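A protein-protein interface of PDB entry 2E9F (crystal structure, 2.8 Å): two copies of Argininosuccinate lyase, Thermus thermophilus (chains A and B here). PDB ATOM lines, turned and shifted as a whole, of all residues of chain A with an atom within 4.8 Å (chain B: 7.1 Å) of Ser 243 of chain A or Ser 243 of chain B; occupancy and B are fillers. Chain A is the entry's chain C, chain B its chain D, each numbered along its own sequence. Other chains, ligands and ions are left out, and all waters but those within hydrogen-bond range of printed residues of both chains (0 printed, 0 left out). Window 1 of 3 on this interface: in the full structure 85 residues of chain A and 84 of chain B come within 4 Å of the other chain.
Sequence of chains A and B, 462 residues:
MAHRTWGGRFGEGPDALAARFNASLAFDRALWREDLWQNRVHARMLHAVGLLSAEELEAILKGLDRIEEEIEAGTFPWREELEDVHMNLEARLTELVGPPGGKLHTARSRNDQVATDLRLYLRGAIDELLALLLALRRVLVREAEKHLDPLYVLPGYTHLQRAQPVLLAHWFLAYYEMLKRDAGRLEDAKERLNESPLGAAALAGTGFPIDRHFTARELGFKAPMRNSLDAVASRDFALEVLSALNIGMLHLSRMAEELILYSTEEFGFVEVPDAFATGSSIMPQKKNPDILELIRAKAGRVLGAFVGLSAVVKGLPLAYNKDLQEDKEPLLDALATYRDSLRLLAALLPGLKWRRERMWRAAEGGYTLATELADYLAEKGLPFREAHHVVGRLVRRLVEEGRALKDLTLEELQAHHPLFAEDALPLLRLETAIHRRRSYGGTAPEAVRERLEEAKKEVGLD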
ATOM      1  N   LEU A 239      20.149 -20.021  -0.993  1.00  0.00           N
ATOM      2  CA  LEU A 239      20.892 -19.158  -0.097  1.00  0.00           C
ATOM      3  C   LEU A 239      19.967 -18.769   1.042  1.00  0.00           C
ATOM      4  O   LEU A 239      20.365 -18.731   2.203  1.00  0.00           O
ATOM      5  CB  LEU A 239      21.350 -17.926  -0.868  1.00  0.00           C
ATOM      6  CG  LEU A 239      22.799 -17.455  -0.739  1.00  0.00           C
ATOM      7  CD1 LEU A 239      23.737 -18.612  -0.453  1.00  0.00           C
ATOM      8  CD2 LEU A 239      23.174 -16.743  -2.025  1.00  0.00           C
ATOM      9  N   GLU A 240      18.715 -18.499   0.698  1.00  0.00           N
ATOM     10  CA  GLU A 240      17.722 -18.122   1.689  1.00  0.00           C
ATOM     11  C   GLU A 240      17.472 -19.267   2.684  1.00  0.00           C
ATOM     12  O   GLU A 240      17.504 -19.066   3.896  1.00  0.00           O
ATOM     13  CB  GLU A 240      16.422 -17.704   0.984  1.00  0.00           C
ATOM     14  CG  GLU A 240      15.248 -17.401   1.923  1.00  0.00           C
ATOM     15  CD  GLU A 240      14.133 -16.581   1.271  1.00  0.00           C
ATOM     16  OE1 GLU A 240      13.797 -16.833   0.088  1.00  0.00           O
ATOM     17  OE2 GLU A 240      13.585 -15.690   1.960  1.00  0.00           O
ATOM     18  N   VAL A 241      17.237 -20.468   2.171  1.00  0.00           N
ATOM     19  CA  VAL A 241      16.986 -21.628   3.022  1.00  0.00           C
ATOM     20  C   VAL A 241      18.167 -21.891   3.969  1.00  0.00           C
ATOM     21  O   VAL A 241      17.977 -22.129   5.167  1.00  0.00           O
ATOM     22  CB  VAL A 241      16.709 -22.899   2.160  1.00  0.00           C
ATOM     23  CG1 VAL A 241      16.508 -24.109   3.039  1.00  0.00           C
ATOM     24  CG2 VAL A 241      15.474 -22.690   1.306  1.00  0.00           C
ATOM     25  N   LEU A 242      19.387 -21.836   3.440  1.00  0.00           N
ATOM     26  CA  LEU A 242      20.573 -22.086   4.258  1.00  0.00           C
ATOM     27  C   LEU A 242      20.667 -21.121   5.423  1.00  0.00           C
ATOM     28  O   LEU A 242      21.026 -21.508   6.539  1.00  0.00           O
ATOM     29  CB  LEU A 242      21.841 -21.984   3.405  1.00  0.00           C
ATOM     30  CG  LEU A 242      22.242 -23.241   2.629  1.00  0.00           C
ATOM     31  CD1 LEU A 242      23.499 -22.954   1.830  1.00  0.00           C
ATOM     32  CD2 LEU A 242      22.460 -24.398   3.600  1.00  0.00           C
ATOM     33  N   SER A 243      20.340 -19.861   5.141  1.00  0.00           N
ATOM     34  CA  SER A 243      20.365 -18.786   6.125  1.00  0.00           C
ATOM     35  C   SER A 243      19.420 -19.088   7.268  1.00  0.00           C
ATOM     36  O   SER A 243      19.762 -18.919   8.435  1.00  0.00           O
ATOM     37  CB  SER A 243      19.958 -17.469   5.470  1.00  0.00           C
ATOM     38  OG  SER A 243      19.944 -16.427   6.427  1.00  0.00           O
ATOM     39  N   ALA A 244      18.218 -19.527   6.911  1.00  0.00           N
ATOM     40  CA  ALA A 244      17.209 -19.881   7.895  1.00  0.00           C
ATOM     41  C   ALA A 244      17.763 -21.045   8.712  1.00  0.00           C
ATOM     42  O   ALA A 244      17.696 -21.029   9.934  1.00  0.00           O
ATOM     43  CB  ALA A 244      15.911 -20.271   7.204  1.00  0.00           C
ATOM     44  N   LEU A 245      18.318 -22.047   8.034  1.00  0.00           N
ATOM     45  CA  LEU A 245      18.908 -23.197   8.715  1.00  0.00           C
ATOM     46  C   LEU A 245      19.993 -22.732   9.684  1.00  0.00           C
ATOM     47  O   LEU A 245      20.011 -23.130  10.843  1.00  0.00           O
ATOM     48  CB  LEU A 245      19.525 -24.171   7.700  1.00  0.00           C
ATOM     49  CG  LEU A 245      18.582 -24.879   6.728  1.00  0.00           C
ATOM     50  CD1 LEU A 245      19.398 -25.692   5.742  1.00  0.00           C
ATOM     51  CD2 LEU A 245      17.616 -25.777   7.489  1.00  0.00           C
ATOM     52  N   ASN A 246      20.900 -21.894   9.193  1.00  0.00           N
ATOM     53  CA  ASN A 246      21.990 -21.364  10.003  1.00  0.00           C
ATOM     54  C   ASN A 246      21.488 -20.658  11.269  1.00  0.00           C
ATOM     55  O   ASN A 246      21.938 -20.947  12.374  1.00  0.00           O
ATOM     56  CB  ASN A 246      22.829 -20.403   9.157  1.00  0.00           C
ATOM     57  CG  ASN A 246      23.774 -19.563   9.987  1.00  0.00           C
ATOM     58  OD1 ASN A 246      23.589 -18.350  10.127  1.00  0.00           O
ATOM     59  ND2 ASN A 246      24.792 -20.205  10.551  1.00  0.00           N
ATOM     60  N   ILE A 247      20.557 -19.725  11.103  1.00  0.00           N
ATOM     61  CA  ILE A 247      19.988 -18.993  12.228  1.00  0.00           C
ATOM     62  C   ILE A 247      19.262 -19.929  13.209  1.00  0.00           C
ATOM     63  O   ILE A 247      19.338 -19.743  14.424  1.00  0.00           O
ATOM     64  CB  ILE A 247      18.996 -17.914  11.730  1.00  0.00           C
ATOM     65  CG1 ILE A 247      19.754 -16.851  10.945  1.00  0.00           C
ATOM     66  CG2 ILE A 247      18.253 -17.281  12.908  1.00  0.00           C
ATOM     67  CD1 ILE A 247      18.869 -15.837  10.276  1.00  0.00           C
ATOM     68  N   PHE A 306      26.469 -21.981   4.159  1.00  0.00           N
ATOM     69  CA  PHE A 306      25.973 -20.700   3.690  1.00  0.00           C
ATOM     70  C   PHE A 306      27.079 -19.905   2.987  1.00  0.00           C
ATOM     71  O   PHE A 306      26.865 -19.371   1.904  1.00  0.00           O
ATOM     72  CB  PHE A 306      25.427 -19.899   4.871  1.00  0.00           C
ATOM     73  CG  PHE A 306      24.847 -18.565   4.491  1.00  0.00           C
ATOM     74  CD1 PHE A 306      23.605 -18.479   3.872  1.00  0.00           C
ATOM     75  CD2 PHE A 306      25.548 -17.388   4.749  1.00  0.00           C
ATOM     76  CE1 PHE A 306      23.063 -17.241   3.514  1.00  0.00           C
ATOM     77  CE2 PHE A 306      25.012 -16.137   4.391  1.00  0.00           C
ATOM     78  CZ  PHE A 306      23.766 -16.072   3.773  1.00  0.00           C
ATOM     79  N   ARG B 185      12.302 -10.429   0.841  1.00  0.00           N
ATOM     80  CA  ARG B 185      13.069 -10.943   1.980  1.00  0.00           C
ATOM     81  C   ARG B 185      13.133  -9.835   3.037  1.00  0.00           C
ATOM     82  O   ARG B 185      12.913 -10.096   4.220  1.00  0.00           O
ATOM     83  CB  ARG B 185      14.494 -11.332   1.563  1.00  0.00           C
ATOM     84  CG  ARG B 185      14.700 -12.809   1.178  1.00  0.00           C
ATOM     85  CD  ARG B 185      16.152 -13.070   0.711  1.00  0.00           C
ATOM     86  NE  ARG B 185      16.359 -12.725  -0.695  1.00  0.00           N
ATOM     87  CZ  ARG B 185      15.933 -13.477  -1.707  1.00  0.00           C
ATOM     88  NH1 ARG B 185      15.293 -14.614  -1.454  1.00  0.00           N
ATOM     89  NH2 ARG B 185      16.112 -13.081  -2.964  1.00  0.00           N
ATOM     90  N   PHE B 237      17.158 -11.415  14.425  1.00  0.00           N
ATOM     91  CA  PHE B 237      16.625 -10.520  13.408  1.00  0.00           C
ATOM     92  C   PHE B 237      17.786  -9.832  12.702  1.00  0.00           C
ATOM     93  O   PHE B 237      17.787  -9.694  11.483  1.00  0.00           O
ATOM     94  CB  PHE B 237      15.694  -9.461  14.022  1.00  0.00           C
ATOM     95  CG  PHE B 237      16.362  -8.564  15.034  1.00  0.00           C
ATOM     96  CD1 PHE B 237      16.680  -9.036  16.302  1.00  0.00           C
ATOM     97  CD2 PHE B 237      16.681  -7.248  14.711  1.00  0.00           C
ATOM     98  CE1 PHE B 237      17.308  -8.217  17.239  1.00  0.00           C
ATOM     99  CE2 PHE B 237      17.314  -6.410  15.642  1.00  0.00           C
ATOM    100  CZ  PHE B 237      17.628  -6.897  16.910  1.00  0.00           C
ATOM    101  N   ALA B 238      18.777  -9.400  13.473  1.00  0.00           N
ATOM    102  CA  ALA B 238      19.928  -8.725  12.898  1.00  0.00           C
ATOM    103  C   ALA B 238      20.559  -9.670  11.906  1.00  0.00           C
ATOM    104  O   ALA B 238      21.029  -9.261  10.845  1.00  0.00           O
ATOM    105  CB  ALA B 238      20.920  -8.371  13.978  1.00  0.00           C
ATOM    106  N   LEU B 239      20.546 -10.948  12.256  1.00  0.00           N
ATOM    107  CA  LEU B 239      21.117 -11.981  11.404  1.00  0.00           C
ATOM    108  C   LEU B 239      20.262 -12.224  10.166  1.00  0.00           C
ATOM    109  O   LEU B 239      20.785 -12.496   9.092  1.00  0.00           O
ATOM    110  CB  LEU B 239      21.276 -13.270  12.206  1.00  0.00           C
ATOM    111  CG  LEU B 239      22.671 -13.896  12.291  1.00  0.00           C
ATOM    112  CD1 LEU B 239      23.762 -12.845  12.411  1.00  0.00           C
ATOM    113  CD2 LEU B 239      22.688 -14.836  13.481  1.00  0.00           C
ATOM    114  N   GLU B 240      18.945 -12.119  10.312  1.00  0.00           N
ATOM    115  CA  GLU B 240      18.061 -12.331   9.173  1.00  0.00           C
ATOM    116  C   GLU B 240      18.204 -11.177   8.192  1.00  0.00           C
ATOM    117  O   GLU B 240      18.250 -11.382   6.978  1.00  0.00           O
ATOM    118  CB  GLU B 240      16.612 -12.430   9.614  1.00  0.00           C
ATOM    119  CG  GLU B 240      15.729 -12.964   8.526  1.00  0.00           C
ATOM    120  CD  GLU B 240      14.256 -12.824   8.834  1.00  0.00           C
ATOM    121  OE1 GLU B 240      13.823 -13.222   9.939  1.00  0.00           O
ATOM    122  OE2 GLU B 240      13.528 -12.316   7.951  1.00  0.00           O
ATOM    123  N   VAL B 241      18.270  -9.958   8.719  1.00  0.00           N
ATOM    124  CA  VAL B 241      18.430  -8.793   7.870  1.00  0.00           C
ATOM    125  C   VAL B 241      19.741  -8.892   7.103  1.00  0.00           C
ATOM    126  O   VAL B 241      19.784  -8.634   5.907  1.00  0.00           O
ATOM    127  CB  VAL B 241      18.447  -7.504   8.694  1.00  0.00           C
ATOM    128  CG1 VAL B 241      18.614  -6.301   7.774  1.00  0.00           C
ATOM    129  CG2 VAL B 241      17.166  -7.397   9.495  1.00  0.00           C
ATOM    130  N   LEU B 242      20.810  -9.265   7.802  1.00  0.00           N
ATOM    131  CA  LEU B 242      22.125  -9.394   7.179  1.00  0.00           C
ATOM    132  C   LEU B 242      22.129 -10.369   6.004  1.00  0.00           C
ATOM    133  O   LEU B 242      22.786 -10.124   4.990  1.00  0.00           O
ATOM    134  CB  LEU B 242      23.175  -9.821   8.214  1.00  0.00           C
ATOM    135  CG  LEU B 242      23.947  -8.694   8.918  1.00  0.00           C
ATOM    136  CD1 LEU B 242      24.886  -9.271   9.958  1.00  0.00           C
ATOM    137  CD2 LEU B 242      24.731  -7.889   7.902  1.00  0.00           C
ATOM    138  N   SER B 243      21.398 -11.472   6.149  1.00  0.00           N
ATOM    139  CA  SER B 243      21.306 -12.481   5.102  1.00  0.00           C
ATOM    140  C   SER B 243      20.657 -11.888   3.852  1.00  0.00           C
ATOM    141  O   SER B 243      21.097 -12.137   2.725  1.00  0.00           O
ATOM    142  CB  SER B 243      20.487 -13.665   5.601  1.00  0.00           C
ATOM    143  OG  SER B 243      20.130 -14.523   4.534  1.00  0.00           O
ATOM    144  N   ALA B 244      19.604 -11.103   4.061  1.00  0.00           N
ATOM    145  CA  ALA B 244      18.915 -10.461   2.958  1.00  0.00           C
ATOM    146  C   ALA B 244      19.897  -9.530   2.239  1.00  0.00           C
ATOM    147  O   ALA B 244      19.990  -9.540   1.009  1.00  0.00           O
ATOM    148  CB  ALA B 244      17.724  -9.680   3.473  1.00  0.00           C
ATOM    149  N   LEU B 245      20.635  -8.729   3.006  1.00  0.00           N
ATOM    150  CA  LEU B 245      21.614  -7.827   2.420  1.00  0.00           C
ATOM    151  C   LEU B 245      22.627  -8.609   1.581  1.00  0.00           C
ATOM    152  O   LEU B 245      23.021  -8.175   0.497  1.00  0.00           O
ATOM    153  CB  LEU B 245      22.330  -7.061   3.520  1.00  0.00           C
ATOM    154  CG  LEU B 245      21.448  -6.084   4.298  1.00  0.00           C
ATOM    155  CD1 LEU B 245      22.274  -5.455   5.416  1.00  0.00           C
ATOM    156  CD2 LEU B 245      20.889  -5.015   3.360  1.00  0.00           C
ATOM    157  N   ASN B 246      23.038  -9.767   2.090  1.00  0.00           N
ATOM    158  CA  ASN B 246      23.992 -10.639   1.408  1.00  0.00           C
ATOM    159  C   ASN B 246      23.456 -11.048   0.034  1.00  0.00           C
ATOM    160  O   ASN B 246      24.079 -10.792  -0.999  1.00  0.00           O
ATOM    161  CB  ASN B 246      24.246 -11.891   2.261  1.00  0.00           C
ATOM    162  CG  ASN B 246      25.217 -12.864   1.607  1.00  0.00           C
ATOM    163  OD1 ASN B 246      24.957 -14.068   1.546  1.00  0.00           O
ATOM    164  ND2 ASN B 246      26.344 -12.350   1.123  1.00  0.00           N
ATOM    165  N   ILE B 247      22.295 -11.688   0.028  1.00  0.00           N
ATOM    166  CA  ILE B 247      21.691 -12.121  -1.218  1.00  0.00           C
ATOM    167  C   ILE B 247      21.487 -10.915  -2.152  1.00  0.00           C
ATOM    168  O   ILE B 247      21.602 -11.028  -3.372  1.00  0.00           O
ATOM    169  CB  ILE B 247      20.356 -12.840  -0.928  1.00  0.00           C
ATOM    170  CG1 ILE B 247      20.618 -14.039  -0.016  1.00  0.00           C
ATOM    171  CG2 ILE B 247      19.733 -13.324  -2.207  1.00  0.00           C
ATOM    172  CD1 ILE B 247      19.372 -14.731   0.490  1.00  0.00           C
ATOM    173  N   GLY B 248      21.212  -9.754  -1.562  1.00  0.00           N
ATOM    174  CA  GLY B 248      21.002  -8.547  -2.342  1.00  0.00           C
ATOM    175  C   GLY B 248      22.236  -8.099  -3.101  1.00  0.00           C
ATOM    176  O   GLY B 248      22.161  -7.807  -4.297  1.00  0.00           O
ATOM    177  N   MET B 249      23.369  -8.024  -2.407  1.00  0.00           N
ATOM    178  CA  MET B 249      24.622  -7.630  -3.041  1.00  0.00           C
ATOM    179  C   MET B 249      25.025  -8.696  -4.056  1.00  0.00           C
ATOM    180  O   MET B 249      25.546  -8.373  -5.121  1.00  0.00           O
ATOM    181  CB  MET B 249      25.729  -7.491  -1.999  1.00  0.00           C
ATOM    182  CG  MET B 249      25.629  -6.266  -1.124  1.00  0.00           C
ATOM    183  SD  MET B 249      25.974  -4.752  -2.022  1.00  0.00           S
ATOM    184  CE  MET B 249      27.606  -5.079  -2.622  1.00  0.00           C
ATOM    185  N   LEU B 250      24.782  -9.966  -3.720  1.00  0.00           N
ATOM    186  CA  LEU B 250      25.123 -11.077  -4.614  1.00  0.00           C
ATOM    187  C   LEU B 250      24.385 -10.954  -5.947  1.00  0.00           C
ATOM    188  O   LEU B 250      24.956 -11.224  -7.006  1.00  0.00           O
ATOM    189  CB  LEU B 250      24.810 -12.434  -3.953  1.00  0.00           C
ATOM    190  CG  LEU B 250      25.623 -12.823  -2.704  1.00  0.00           C
ATOM    191  CD1 LEU B 250      25.213 -14.195  -2.243  1.00  0.00           C
ATOM    192  CD2 LEU B 250      27.118 -12.792  -3.001  1.00  0.00           C
ATOM    193  N   VAL B 302      29.762  -7.820   3.126  1.00  0.00           N
ATOM    194  CA  VAL B 302      28.451  -8.074   3.704  1.00  0.00           C
ATOM    195  C   VAL B 302      28.403  -9.543   4.128  1.00  0.00           C
ATOM    196  O   VAL B 302      27.864  -9.879   5.184  1.00  0.00           O
ATOM    197  CB  VAL B 302      27.309  -7.760   2.712  1.00  0.00           C
ATOM    198  CG1 VAL B 302      25.974  -8.118   3.330  1.00  0.00           C
ATOM    199  CG2 VAL B 302      27.314  -6.283   2.370  1.00  0.00           C
ATOM    200  N   PHE B 306      27.806 -11.221   8.053  1.00  0.00           N
ATOM    201  CA  PHE B 306      26.867 -12.257   8.462  1.00  0.00           C
ATOM    202  C   PHE B 306      27.645 -13.324   9.234  1.00  0.00           C
ATOM    203  O   PHE B 306      27.182 -13.872  10.237  1.00  0.00           O
ATOM    204  CB  PHE B 306      26.239 -12.875   7.214  1.00  0.00           C
ATOM    205  CG  PHE B 306      25.234 -13.960   7.490  1.00  0.00           C
ATOM    206  CD1 PHE B 306      23.895 -13.654   7.699  1.00  0.00           C
ATOM    207  CD2 PHE B 306      25.612 -15.295   7.478  1.00  0.00           C
ATOM    208  CE1 PHE B 306      22.945 -14.665   7.886  1.00  0.00           C
ATOM    209  CE2 PHE B 306      24.669 -16.311   7.666  1.00  0.00           C
ATOM    210  CZ  PHE B 306      23.335 -15.994   7.867  1.00  0.00           C
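The side-chain carboxylate of Glu 240 of chain A is in salt-bridge range of the guanidinium group of Arg 185 of chain B (3.1 Å).
OG of Ser 243 of chain B is in hydrogen-bond range of OG of Ser 243 of chain A.
Among the printed residues, merely in contact across the chains: Phe 306 of chain A with Asn 246 of chain B (3.2 Å), Phe 306 of chain A with Phe 306 of chain B (3.2 Å), Leu 239 of chain A with Leu 250 of chain B (3.3 Å), Asn 246 of chain A with Phe 306 of chain B (3.3 Å), Ser 243 of chain A with Phe 306 of chain B (3.7 Å), Ile 247 of chain A with Glu 240 of chain B (3.7 Å), Glu 240 of chain A with Ile 247 of chain B (3.8 Å), Ile 247 of chain A with Leu 239 of chain B (3.9 Å) and Leu 239 of chain A with Ile 247 of chain B (3.996 Å).
Ser 243 of chain A touches just these residues of chain B: Ser 243 (2.7 Å) and Phe 306 (3.7 Å).
Of chain A, only Ser 243 (2.7 Å) comes within 4 Å of Ser 243 of chain B.
Of the printed residues of chain A, Glu 240 of chain B touches Ile 247 (3.7 Å).
Printed residues of chain B within 4 Å of Asn 246 of chain A: Phe 306 (3.3 Å).
Printed residues of chain A within 4 Å of Leu 250 of chain B: Leu 239.
Of the printed residues of chain A, Ile 247 of chain B touches Leu 239 (3.996 Å) and Glu 240 (3.8 Å).
Val 241 of chain B touches none of the printed residues of chain A.
The nearest residue of chain A that does not touch Ser 243 of chain B is Phe 306 of chain A (4.02 Å).
Of the 10 printed residues of chain A, 6 touch a printed residue of chain B.
Hydrophobic or aromatic side chains of chain A within 4 Å of the printed part of chain B: Leu 239, Ile 247 and Phe 306.
Along chain A the printed residues that touch a printed residue of chain B span positions 239 to 306.
Among the printed residues, 11 pairs touch across the chains.
Leu 239 of chain A touches Ile 247 of chain B, and with the chains exchanged Ile 247 of chain A touches Leu 239 of chain B.
Glu 240 of chain A touches Ile 247 of chain B, and with the chains exchanged Ile 247 of chain A touches Glu 240 of chain B.
Ser 243 of chain B touches its own counterpart, Ser 243 of chain A.
Asn 246 of chain A touches Phe 306 of chain B, and with the chains exchanged Phe 306 of chain A touches Asn 246 of chain B.
Of the 11 pairs that touch across the chains among the printed residues, 8 have their exchanged pair printed and touching as well.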
